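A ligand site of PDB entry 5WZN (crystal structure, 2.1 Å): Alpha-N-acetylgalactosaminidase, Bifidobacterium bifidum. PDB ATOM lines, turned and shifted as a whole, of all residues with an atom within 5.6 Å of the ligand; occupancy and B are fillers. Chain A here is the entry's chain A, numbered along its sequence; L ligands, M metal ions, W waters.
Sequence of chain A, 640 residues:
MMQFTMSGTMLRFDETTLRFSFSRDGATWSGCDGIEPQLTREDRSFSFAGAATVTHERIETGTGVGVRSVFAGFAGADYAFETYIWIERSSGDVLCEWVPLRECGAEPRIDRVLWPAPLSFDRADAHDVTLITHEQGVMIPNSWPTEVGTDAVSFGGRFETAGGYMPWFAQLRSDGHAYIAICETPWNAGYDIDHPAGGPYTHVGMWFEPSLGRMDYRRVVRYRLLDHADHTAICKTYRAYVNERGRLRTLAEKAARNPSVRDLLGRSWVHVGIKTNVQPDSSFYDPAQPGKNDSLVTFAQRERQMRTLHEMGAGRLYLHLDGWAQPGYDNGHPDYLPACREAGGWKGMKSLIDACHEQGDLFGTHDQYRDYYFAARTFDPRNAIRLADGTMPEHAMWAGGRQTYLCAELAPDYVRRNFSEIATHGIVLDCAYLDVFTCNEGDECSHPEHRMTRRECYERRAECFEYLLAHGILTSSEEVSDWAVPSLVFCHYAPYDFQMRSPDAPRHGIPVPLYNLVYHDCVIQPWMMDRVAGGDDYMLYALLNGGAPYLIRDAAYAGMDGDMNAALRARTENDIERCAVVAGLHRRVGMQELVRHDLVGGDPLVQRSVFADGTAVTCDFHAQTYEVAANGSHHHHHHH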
ATOM      1  N   HIS A 271     -23.876 -17.126 -22.316  1.00  0.00           N
ATOM      2  CA  HIS A 271     -22.679 -17.291 -21.500  1.00  0.00           C
ATOM      3  C   HIS A 271     -22.838 -16.475 -20.193  1.00  0.00           C
ATOM      4  O   HIS A 271     -22.755 -15.259 -20.224  1.00  0.00           O
ATOM      5  CB  HIS A 271     -21.448 -16.851 -22.304  1.00  0.00           C
ATOM      6  CG  HIS A 271     -20.178 -17.072 -21.567  1.00  0.00           C
ATOM      7  ND1 HIS A 271     -19.724 -16.206 -20.575  1.00  0.00           N
ATOM      8  CD2 HIS A 271     -19.286 -18.105 -21.598  1.00  0.00           C
ATOM      9  CE1 HIS A 271     -18.620 -16.689 -20.028  1.00  0.00           C
ATOM     10  NE2 HIS A 271     -18.325 -17.836 -20.640  1.00  0.00           N
ATOM     11  N   TYR A 329     -15.726 -19.492  -9.845  1.00  0.00           N
ATOM     12  CA  TYR A 329     -15.053 -19.342 -11.106  1.00  0.00           C
ATOM     13  C   TYR A 329     -13.527 -19.092 -10.924  1.00  0.00           C
ATOM     14  O   TYR A 329     -13.108 -18.267 -10.117  1.00  0.00           O
ATOM     15  CB  TYR A 329     -15.676 -18.203 -11.889  1.00  0.00           C
ATOM     16  CG  TYR A 329     -15.120 -18.068 -13.290  1.00  0.00           C
ATOM     17  CD1 TYR A 329     -15.554 -18.938 -14.302  1.00  0.00           C
ATOM     18  CD2 TYR A 329     -14.139 -17.115 -13.602  1.00  0.00           C
ATOM     19  CE1 TYR A 329     -15.072 -18.812 -15.577  1.00  0.00           C
ATOM     20  CE2 TYR A 329     -13.608 -16.994 -14.897  1.00  0.00           C
ATOM     21  CZ  TYR A 329     -14.081 -17.849 -15.880  1.00  0.00           C
ATOM     22  OH  TYR A 329     -13.637 -17.732 -17.180  1.00  0.00           O
ATOM     23  N   ASP A 330     -12.752 -19.842 -11.715  1.00  0.00           N
ATOM     24  CA  ASP A 330     -11.309 -19.773 -11.684  1.00  0.00           C
ATOM     25  C   ASP A 330     -10.704 -19.983 -10.296  1.00  0.00           C
ATOM     26  O   ASP A 330      -9.693 -19.351  -9.997  1.00  0.00           O
ATOM     27  CB  ASP A 330     -10.825 -18.442 -12.305  1.00  0.00           C
ATOM     28  CG  ASP A 330     -10.748 -18.501 -13.855  1.00  0.00           C
ATOM     29  OD1 ASP A 330     -10.909 -19.600 -14.470  1.00  0.00           O
ATOM     30  OD2 ASP A 330     -10.456 -17.436 -14.454  1.00  0.00           O
ATOM     31  N   HIS A 366     -18.440 -24.656 -18.010  1.00  0.00           N
ATOM     32  CA  HIS A 366     -17.112 -24.059 -18.150  1.00  0.00           C
ATOM     33  C   HIS A 366     -16.178 -24.786 -17.158  1.00  0.00           C
ATOM     34  O   HIS A 366     -16.367 -24.720 -15.946  1.00  0.00           O
ATOM     35  CB  HIS A 366     -17.146 -22.576 -17.802  1.00  0.00           C
ATOM     36  CG  HIS A 366     -15.814 -21.878 -17.933  1.00  0.00           C
ATOM     37  ND1 HIS A 366     -15.615 -20.787 -18.765  1.00  0.00           N
ATOM     38  CD2 HIS A 366     -14.617 -22.112 -17.334  1.00  0.00           C
ATOM     39  CE1 HIS A 366     -14.369 -20.369 -18.651  1.00  0.00           C
ATOM     40  NE2 HIS A 366     -13.737 -21.184 -17.819  1.00  0.00           N
ATOM     41  N   GLN A 368     -11.782 -26.254 -16.476  1.00  0.00           N
ATOM     42  CA  GLN A 368     -10.402 -25.707 -16.628  1.00  0.00           C
ATOM     43  C   GLN A 368      -9.418 -26.778 -16.140  1.00  0.00           C
ATOM     44  O   GLN A 368      -9.529 -27.220 -15.004  1.00  0.00           O
ATOM     45  CB  GLN A 368     -10.217 -24.442 -15.738  1.00  0.00           C
ATOM     46  CG  GLN A 368      -8.760 -23.965 -15.557  1.00  0.00           C
ATOM     47  CD  GLN A 368      -8.123 -23.402 -16.836  1.00  0.00           C
ATOM     48  OE1 GLN A 368      -7.110 -23.958 -17.347  1.00  0.00           O
ATOM     49  NE2 GLN A 368      -8.669 -22.302 -17.361  1.00  0.00           N
ATOM     50  N   ASP A 371      -4.749 -24.379 -15.633  1.00  0.00           N
ATOM     51  CA  ASP A 371      -4.436 -23.584 -14.401  1.00  0.00           C
ATOM     52  C   ASP A 371      -4.529 -24.516 -13.174  1.00  0.00           C
ATOM     53  O   ASP A 371      -5.512 -25.263 -13.024  1.00  0.00           O
ATOM     54  CB  ASP A 371      -5.347 -22.379 -14.225  1.00  0.00           C
ATOM     55  CG  ASP A 371      -5.282 -21.395 -15.448  1.00  0.00           C
ATOM     56  OD1 ASP A 371      -4.223 -21.208 -16.084  1.00  0.00           O
ATOM     57  OD2 ASP A 371      -6.340 -20.791 -15.818  1.00  0.00           O
ATOM     58  N   TYR A 373      -4.227 -24.429  -9.125  1.00  0.00           N
ATOM     59  CA  TYR A 373      -4.235 -23.435  -8.054  1.00  0.00           C
ATOM     60  C   TYR A 373      -3.662 -24.049  -6.795  1.00  0.00           C
ATOM     61  O   TYR A 373      -3.955 -25.207  -6.450  1.00  0.00           O
ATOM     62  CB  TYR A 373      -5.667 -22.908  -7.786  1.00  0.00           C
ATOM     63  CG  TYR A 373      -6.114 -22.037  -8.904  1.00  0.00           C
ATOM     64  CD1 TYR A 373      -5.798 -20.676  -8.901  1.00  0.00           C
ATOM     65  CD2 TYR A 373      -6.809 -22.568 -10.021  1.00  0.00           C
ATOM     66  CE1 TYR A 373      -6.181 -19.874  -9.964  1.00  0.00           C
ATOM     67  CE2 TYR A 373      -7.202 -21.759 -11.115  1.00  0.00           C
ATOM     68  CZ  TYR A 373      -6.880 -20.436 -11.061  1.00  0.00           C
ATOM     69  OH  TYR A 373      -7.264 -19.614 -12.100  1.00  0.00           O
ATOM     70  N   TRP A 398      -5.340 -14.772 -11.853  1.00  0.00           N
ATOM     71  CA  TRP A 398      -6.812 -14.986 -11.899  1.00  0.00           C
ATOM     72  C   TRP A 398      -7.519 -14.996 -10.563  1.00  0.00           C
ATOM     73  O   TRP A 398      -6.897 -14.813  -9.514  1.00  0.00           O
ATOM     74  CB  TRP A 398      -7.156 -16.256 -12.695  1.00  0.00           C
ATOM     75  CG  TRP A 398      -6.489 -16.252 -14.009  1.00  0.00           C
ATOM     76  CD1 TRP A 398      -5.504 -17.108 -14.423  1.00  0.00           C
ATOM     77  CD2 TRP A 398      -6.693 -15.313 -15.090  1.00  0.00           C
ATOM     78  NE1 TRP A 398      -5.086 -16.788 -15.689  1.00  0.00           N
ATOM     79  CE2 TRP A 398      -5.794 -15.697 -16.132  1.00  0.00           C
ATOM     80  CE3 TRP A 398      -7.578 -14.238 -15.295  1.00  0.00           C
ATOM     81  CZ2 TRP A 398      -5.758 -15.029 -17.424  1.00  0.00           C
ATOM     82  CZ3 TRP A 398      -7.524 -13.538 -16.534  1.00  0.00           C
ATOM     83  CH2 TRP A 398      -6.626 -13.955 -17.602  1.00  0.00           C
ATOM     84  N   TYR A 433     -16.790 -27.369 -21.915  1.00  0.00           N
ATOM     85  CA  TYR A 433     -15.780 -26.386 -22.302  1.00  0.00           C
ATOM     86  C   TYR A 433     -14.534 -26.616 -21.429  1.00  0.00           C
ATOM     87  O   TYR A 433     -14.652 -26.499 -20.195  1.00  0.00           O
ATOM     88  CB  TYR A 433     -16.328 -25.008 -21.960  1.00  0.00           C
ATOM     89  CG  TYR A 433     -15.458 -23.836 -22.353  1.00  0.00           C
ATOM     90  CD1 TYR A 433     -15.414 -23.405 -23.660  1.00  0.00           C
ATOM     91  CD2 TYR A 433     -14.722 -23.102 -21.354  1.00  0.00           C
ATOM     92  CE1 TYR A 433     -14.639 -22.274 -24.050  1.00  0.00           C
ATOM     93  CE2 TYR A 433     -13.921 -22.011 -21.713  1.00  0.00           C
ATOM     94  CZ  TYR A 433     -13.894 -21.580 -23.047  1.00  0.00           C
ATOM     95  OH  TYR A 433     -13.159 -20.481 -23.381  1.00  0.00           O
ATOM     96  N   ASP A 435     -11.392 -24.826 -20.884  1.00  0.00           N
ATOM     97  CA  ASP A 435     -10.792 -23.502 -21.114  1.00  0.00           C
ATOM     98  C   ASP A 435      -9.320 -23.557 -21.523  1.00  0.00           C
ATOM     99  O   ASP A 435      -8.638 -24.566 -21.267  1.00  0.00           O
ATOM    100  CB  ASP A 435     -10.977 -22.641 -19.879  1.00  0.00           C
ATOM    101  CG  ASP A 435     -11.031 -21.155 -20.222  1.00  0.00           C
ATOM    102  OD1 ASP A 435     -10.931 -20.819 -21.432  1.00  0.00           O
ATOM    103  OD2 ASP A 435     -11.193 -20.339 -19.274  1.00  0.00           O
ATOM    104  N   VAL A 436      -8.879 -22.478 -22.217  1.00  0.00           N
ATOM    105  CA  VAL A 436      -7.486 -22.199 -22.633  1.00  0.00           C
ATOM    106  C   VAL A 436      -6.751 -23.156 -23.570  1.00  0.00           C
ATOM    107  O   VAL A 436      -5.885 -22.721 -24.282  1.00  0.00           O
ATOM    108  CB  VAL A 436      -6.561 -21.823 -21.439  1.00  0.00           C
ATOM    109  CG1 VAL A 436      -7.313 -21.034 -20.365  1.00  0.00           C
ATOM    110  CG2 VAL A 436      -5.922 -23.062 -20.843  1.00  0.00           C
ATOM    111  N   ASN A 440      -4.053 -20.897 -25.800  1.00  0.00           N
ATOM    112  CA  ASN A 440      -2.624 -20.801 -25.353  1.00  0.00           C
ATOM    113  C   ASN A 440      -1.737 -21.905 -25.873  1.00  0.00           C
ATOM    114  O   ASN A 440      -2.210 -23.001 -26.226  1.00  0.00           O
ATOM    115  CB  ASN A 440      -2.544 -20.817 -23.798  1.00  0.00           C
ATOM    116  CG  ASN A 440      -3.224 -19.635 -23.188  1.00  0.00           C
ATOM    117  OD1 ASN A 440      -4.410 -19.365 -23.436  1.00  0.00           O
ATOM    118  ND2 ASN A 440      -2.461 -18.879 -22.425  1.00  0.00           N
ATOM    119  N   GLU A 478     -11.485 -22.416 -25.737  1.00  0.00           N
ATOM    120  CA  GLU A 478     -11.443 -20.971 -25.912  1.00  0.00           C
ATOM    121  C   GLU A 478     -11.480 -20.502 -27.344  1.00  0.00           C
ATOM    122  O   GLU A 478     -12.354 -19.715 -27.703  1.00  0.00           O
ATOM    123  CB  GLU A 478     -10.197 -20.397 -25.198  1.00  0.00           C
ATOM    124  CG  GLU A 478     -10.305 -18.896 -24.944  1.00  0.00           C
ATOM    125  CD  GLU A 478      -9.197 -18.389 -23.977  1.00  0.00           C
ATOM    126  OE1 GLU A 478      -8.360 -19.174 -23.436  1.00  0.00           O
ATOM    127  OE2 GLU A 478      -9.206 -17.195 -23.739  1.00  0.00           O
ATOM    128  N   HIS A 492     -15.468 -20.868 -27.891  1.00  0.00           N
ATOM    129  CA  HIS A 492     -16.071 -19.724 -27.211  1.00  0.00           C
ATOM    130  C   HIS A 492     -16.214 -18.639 -28.293  1.00  0.00           C
ATOM    131  O   HIS A 492     -17.200 -17.903 -28.289  1.00  0.00           O
ATOM    132  CB  HIS A 492     -15.238 -19.287 -26.005  1.00  0.00           C
ATOM    133  CG  HIS A 492     -15.757 -18.025 -25.331  1.00  0.00           C
ATOM    134  ND1 HIS A 492     -16.573 -18.073 -24.223  1.00  0.00           N
ATOM    135  CD2 HIS A 492     -15.571 -16.709 -25.625  1.00  0.00           C
ATOM    136  CE1 HIS A 492     -16.868 -16.835 -23.863  1.00  0.00           C
ATOM    137  NE2 HIS A 492     -16.285 -15.986 -24.702  1.00  0.00           N
ATOM    138  N   TYR A 493     -15.248 -18.568 -29.219  1.00  0.00           N
ATOM    139  CA  TYR A 493     -15.307 -17.708 -30.414  1.00  0.00           C
ATOM    140  C   TYR A 493     -14.090 -17.995 -31.233  1.00  0.00           C
ATOM    141  O   TYR A 493     -13.136 -18.718 -30.795  1.00  0.00           O
ATOM    142  CB  TYR A 493     -15.360 -16.169 -30.112  1.00  0.00           C
ATOM    143  CG  TYR A 493     -14.531 -15.649 -28.913  1.00  0.00           C
ATOM    144  CD1 TYR A 493     -13.354 -16.309 -28.477  1.00  0.00           C
ATOM    145  CD2 TYR A 493     -14.902 -14.434 -28.256  1.00  0.00           C
ATOM    146  CE1 TYR A 493     -12.601 -15.808 -27.429  1.00  0.00           C
ATOM    147  CE2 TYR A 493     -14.152 -13.926 -27.201  1.00  0.00           C
ATOM    148  CZ  TYR A 493     -13.017 -14.617 -26.782  1.00  0.00           C
ATOM    149  OH  TYR A 493     -12.289 -14.177 -25.718  1.00  0.00           O
ATOM    150  N   ALA A 556     -16.402 -12.656 -17.734  1.00  0.00           N
ATOM    151  CA  ALA A 556     -15.932 -13.232 -16.491  1.00  0.00           C
ATOM    152  C   ALA A 556     -15.260 -12.161 -15.615  1.00  0.00           C
ATOM    153  O   ALA A 556     -15.471 -12.125 -14.409  1.00  0.00           O
ATOM    154  CB  ALA A 556     -14.934 -14.348 -16.803  1.00  0.00           C
ATOM    155  N   TYR A 557     -14.413 -11.346 -16.244  1.00  0.00           N
ATOM    156  CA  TYR A 557     -13.648 -10.267 -15.586  1.00  0.00           C
ATOM    157  C   TYR A 557     -13.927  -9.057 -16.472  1.00  0.00           C
ATOM    158  O   TYR A 557     -13.833  -9.176 -17.699  1.00  0.00           O
ATOM    159  CB  TYR A 557     -12.138 -10.557 -15.675  1.00  0.00           C
ATOM    160  CG  TYR A 557     -11.702 -11.844 -15.002  1.00  0.00           C
ATOM    161  CD1 TYR A 557     -11.495 -11.865 -13.631  1.00  0.00           C
ATOM    162  CD2 TYR A 557     -11.506 -13.049 -15.760  1.00  0.00           C
ATOM    163  CE1 TYR A 557     -11.076 -13.024 -12.992  1.00  0.00           C
ATOM    164  CE2 TYR A 557     -11.131 -14.240 -15.120  1.00  0.00           C
ATOM    165  CZ  TYR A 557     -10.895 -14.204 -13.739  1.00  0.00           C
ATOM    166  OH  TYR A 557     -10.534 -15.328 -13.073  1.00  0.00           O
ATOM    167  N   MET A 560     -11.892  -8.069 -20.014  1.00  0.00           N
ATOM    168  CA  MET A 560     -11.263  -9.277 -20.600  1.00  0.00           C
ATOM    169  C   MET A 560     -12.194  -9.936 -21.640  1.00  0.00           C
ATOM    170  O   MET A 560     -13.421  -9.770 -21.556  1.00  0.00           O
ATOM    171  CB  MET A 560     -10.998 -10.323 -19.505  1.00  0.00           C
ATOM    172  CG  MET A 560     -10.144  -9.843 -18.345  1.00  0.00           C
ATOM    173  SD  MET A 560      -8.621  -9.059 -18.948  1.00  0.00           S
ATOM    174  CE  MET A 560      -7.585 -10.470 -19.357  1.00  0.00           C
ATOM    175  N   ASP A 561     -11.610 -10.721 -22.550  1.00  0.00           N
ATOM    176  CA  ASP A 561     -12.381 -11.695 -23.378  1.00  0.00           C
ATOM    177  C   ASP A 561     -13.274 -11.003 -24.424  1.00  0.00           C
ATOM    178  O   ASP A 561     -14.447 -11.376 -24.593  1.00  0.00           O
ATOM    179  CB  ASP A 561     -13.190 -12.715 -22.504  1.00  0.00           C
ATOM    180  CG  ASP A 561     -12.289 -13.525 -21.542  1.00  0.00           C
ATOM    181  OD1 ASP A 561     -11.142 -13.898 -21.979  1.00  0.00           O
ATOM    182  OD2 ASP A 561     -12.698 -13.802 -20.342  1.00  0.00           O
HETATM  183  O1  LIG L   1      -8.964 -18.471 -19.189  1.00  0.00           O
HETATM  184  C1  LIG L   1      -9.594 -17.933 -20.363  1.00  0.00           C
HETATM  185  O2  LIG L   1      -8.749 -16.962 -20.987  1.00  0.00           O
HETATM  186  C2  LIG L   1     -10.900 -17.211 -19.923  1.00  0.00           C
HETATM  187  N1  LIG L   1     -11.594 -16.697 -21.117  1.00  0.00           N
HETATM  188  C3  LIG L   1     -10.627 -16.153 -18.809  1.00  0.00           C
HETATM  189  O3  LIG L   1     -11.879 -15.630 -18.327  1.00  0.00           O
HETATM  190  C4  LIG L   1      -9.879 -16.764 -17.618  1.00  0.00           C
HETATM  191  O4  LIG L   1     -10.717 -17.716 -16.980  1.00  0.00           O
HETATM  192  C5  LIG L   1      -8.653 -17.537 -18.117  1.00  0.00           C
HETATM  193  C6  LIG L   1      -7.965 -18.316 -16.979  1.00  0.00           C
HETATM  194  O5  LIG L   1      -6.741 -18.876 -17.581  1.00  0.00           O
HETATM  195  C7  LIG L   1     -12.757 -17.232 -21.549  1.00  0.00           C
HETATM  196  O6  LIG L   1     -13.301 -18.136 -20.960  1.00  0.00           O
HETATM  197  C8  LIG L   1     -13.437 -16.655 -22.747  1.00  0.00           C
HETATM  198 CA    CA M   1     -16.966 -19.374 -19.689  1.00  0.00          CA
HETATM  199  O   HOH W   1     -15.160 -15.169 -20.421  1.00  0.00           O
HETATM  200  O   HOH W   2      -6.341 -18.069 -22.144  1.00  0.00           O
HETATM  201  O   HOH W   3     -11.052 -20.849 -16.786  1.00  0.00           O
HETATM  202  O   HOH W   4     -15.931 -19.050 -21.378  1.00  0.00           O
HETATM  203  O   HOH W   5     -15.709 -17.526 -18.898  1.00  0.00           O
HETATM  204  O   HOH W   6      -5.171 -18.423 -19.623  1.00  0.00           O
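The side-chain carboxylate of Asp 330 sits at hydrogen-bond distance from an oxygen (O4) of the ligand (2.6 Å). OD2 of Asp 371 sits at hydrogen-bond distance from O5 of the ligand, 2.6 Å away. The side-chain carboxylate of Glu 478 is in hydrogen-bond range of an oxygen (O2) of the ligand, 2.8 Å away. The side-chain carboxylate (OD2) of Asp 561 lies within hydrogen-bond range of an oxygen (O3) of the ligand, 2.8 Å away. The side-chain hydroxyl of Tyr 329 lies within hydrogen-bond range of an oxygen (O4) of the ligand, at 2.9 Å. The indole nitrogen (NE1) of Trp 398 is in hydrogen-bond range of an oxygen (O5) of the ligand, at 3.3 Å. The side-chain hydroxyl (OH) of Tyr 433 sits at hydrogen-bond distance from an oxygen (O6) of the ligand, at 3.4 Å.
The side-chain carboxylate of Asp 330 sits at hydrogen-bond distance from the side-chain hydroxyl of Tyr 557 (2.5 Å). O of Asp 330 lies close to OH of Tyr 373 (3.2 Å). The backbone NH (N) of Asp 371 is in hydrogen-bond range of the side-chain amide oxygen (OE1) of Gln 368. N of Glu 478 sits close to OH of Tyr 433. O of Glu 478 lies within hydrogen-bond range of N of His 492 (3.3 Å). N of Tyr 493 is in hydrogen-bond range of O of Glu 478 (3.5 Å). OH of Tyr 433 sits at hydrogen-bond distance from OD1 of Asp 435. OD2 of Asp 435 is in hydrogen-bond range of NE2 of His 366.
The side-chain carboxylate of Asp 435 sits close to an oxygen (O1) of the ligand (2.9 Å). Residues that only touch the ligand: His 366 (3.4 Å), Gln 368 (3.9 Å), Val 436 (3.3 Å), His 492 (3.5 Å), Ala 556 (3.6 Å) and Tyr 557 (3.6 Å). Hydrophobic or aromatic side chains that line the ligand: Tyr 329, His 366, Trp 398, Tyr 433, Val 436, His 492, Ala 556 and Tyr 557. 14 residues have an atom within 4 Å of the ligand: Tyr 329, Asp 330, His 366, Gln 368, Asp 371, Trp 398, Tyr 433, Asp 435, Val 436, Glu 478, His 492, Ala 556, Tyr 557 and Asp 561. The nearest printed residue that does not touch the ligand is Tyr 493 (4.04 Å).
Water W4 lies within hydrogen-bond range of an oxygen (O6) of the ligand and a ring nitrogen (ND1) of His 492. Water W2 lies within hydrogen-bond range of OE1 of Glu 478 (2.6 Å), OD1 of Asn 440 (2.7 Å) and O2 of the ligand (2.9 Å). Water W3 lies within hydrogen-bond range of OD2 of Asp 435, OD1 of Asp 330, NE2 of Gln 368, NE2 of His 366 and O4 of the ligand. Water W5 bridges OH of Tyr 329 and O6 of the ligand.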
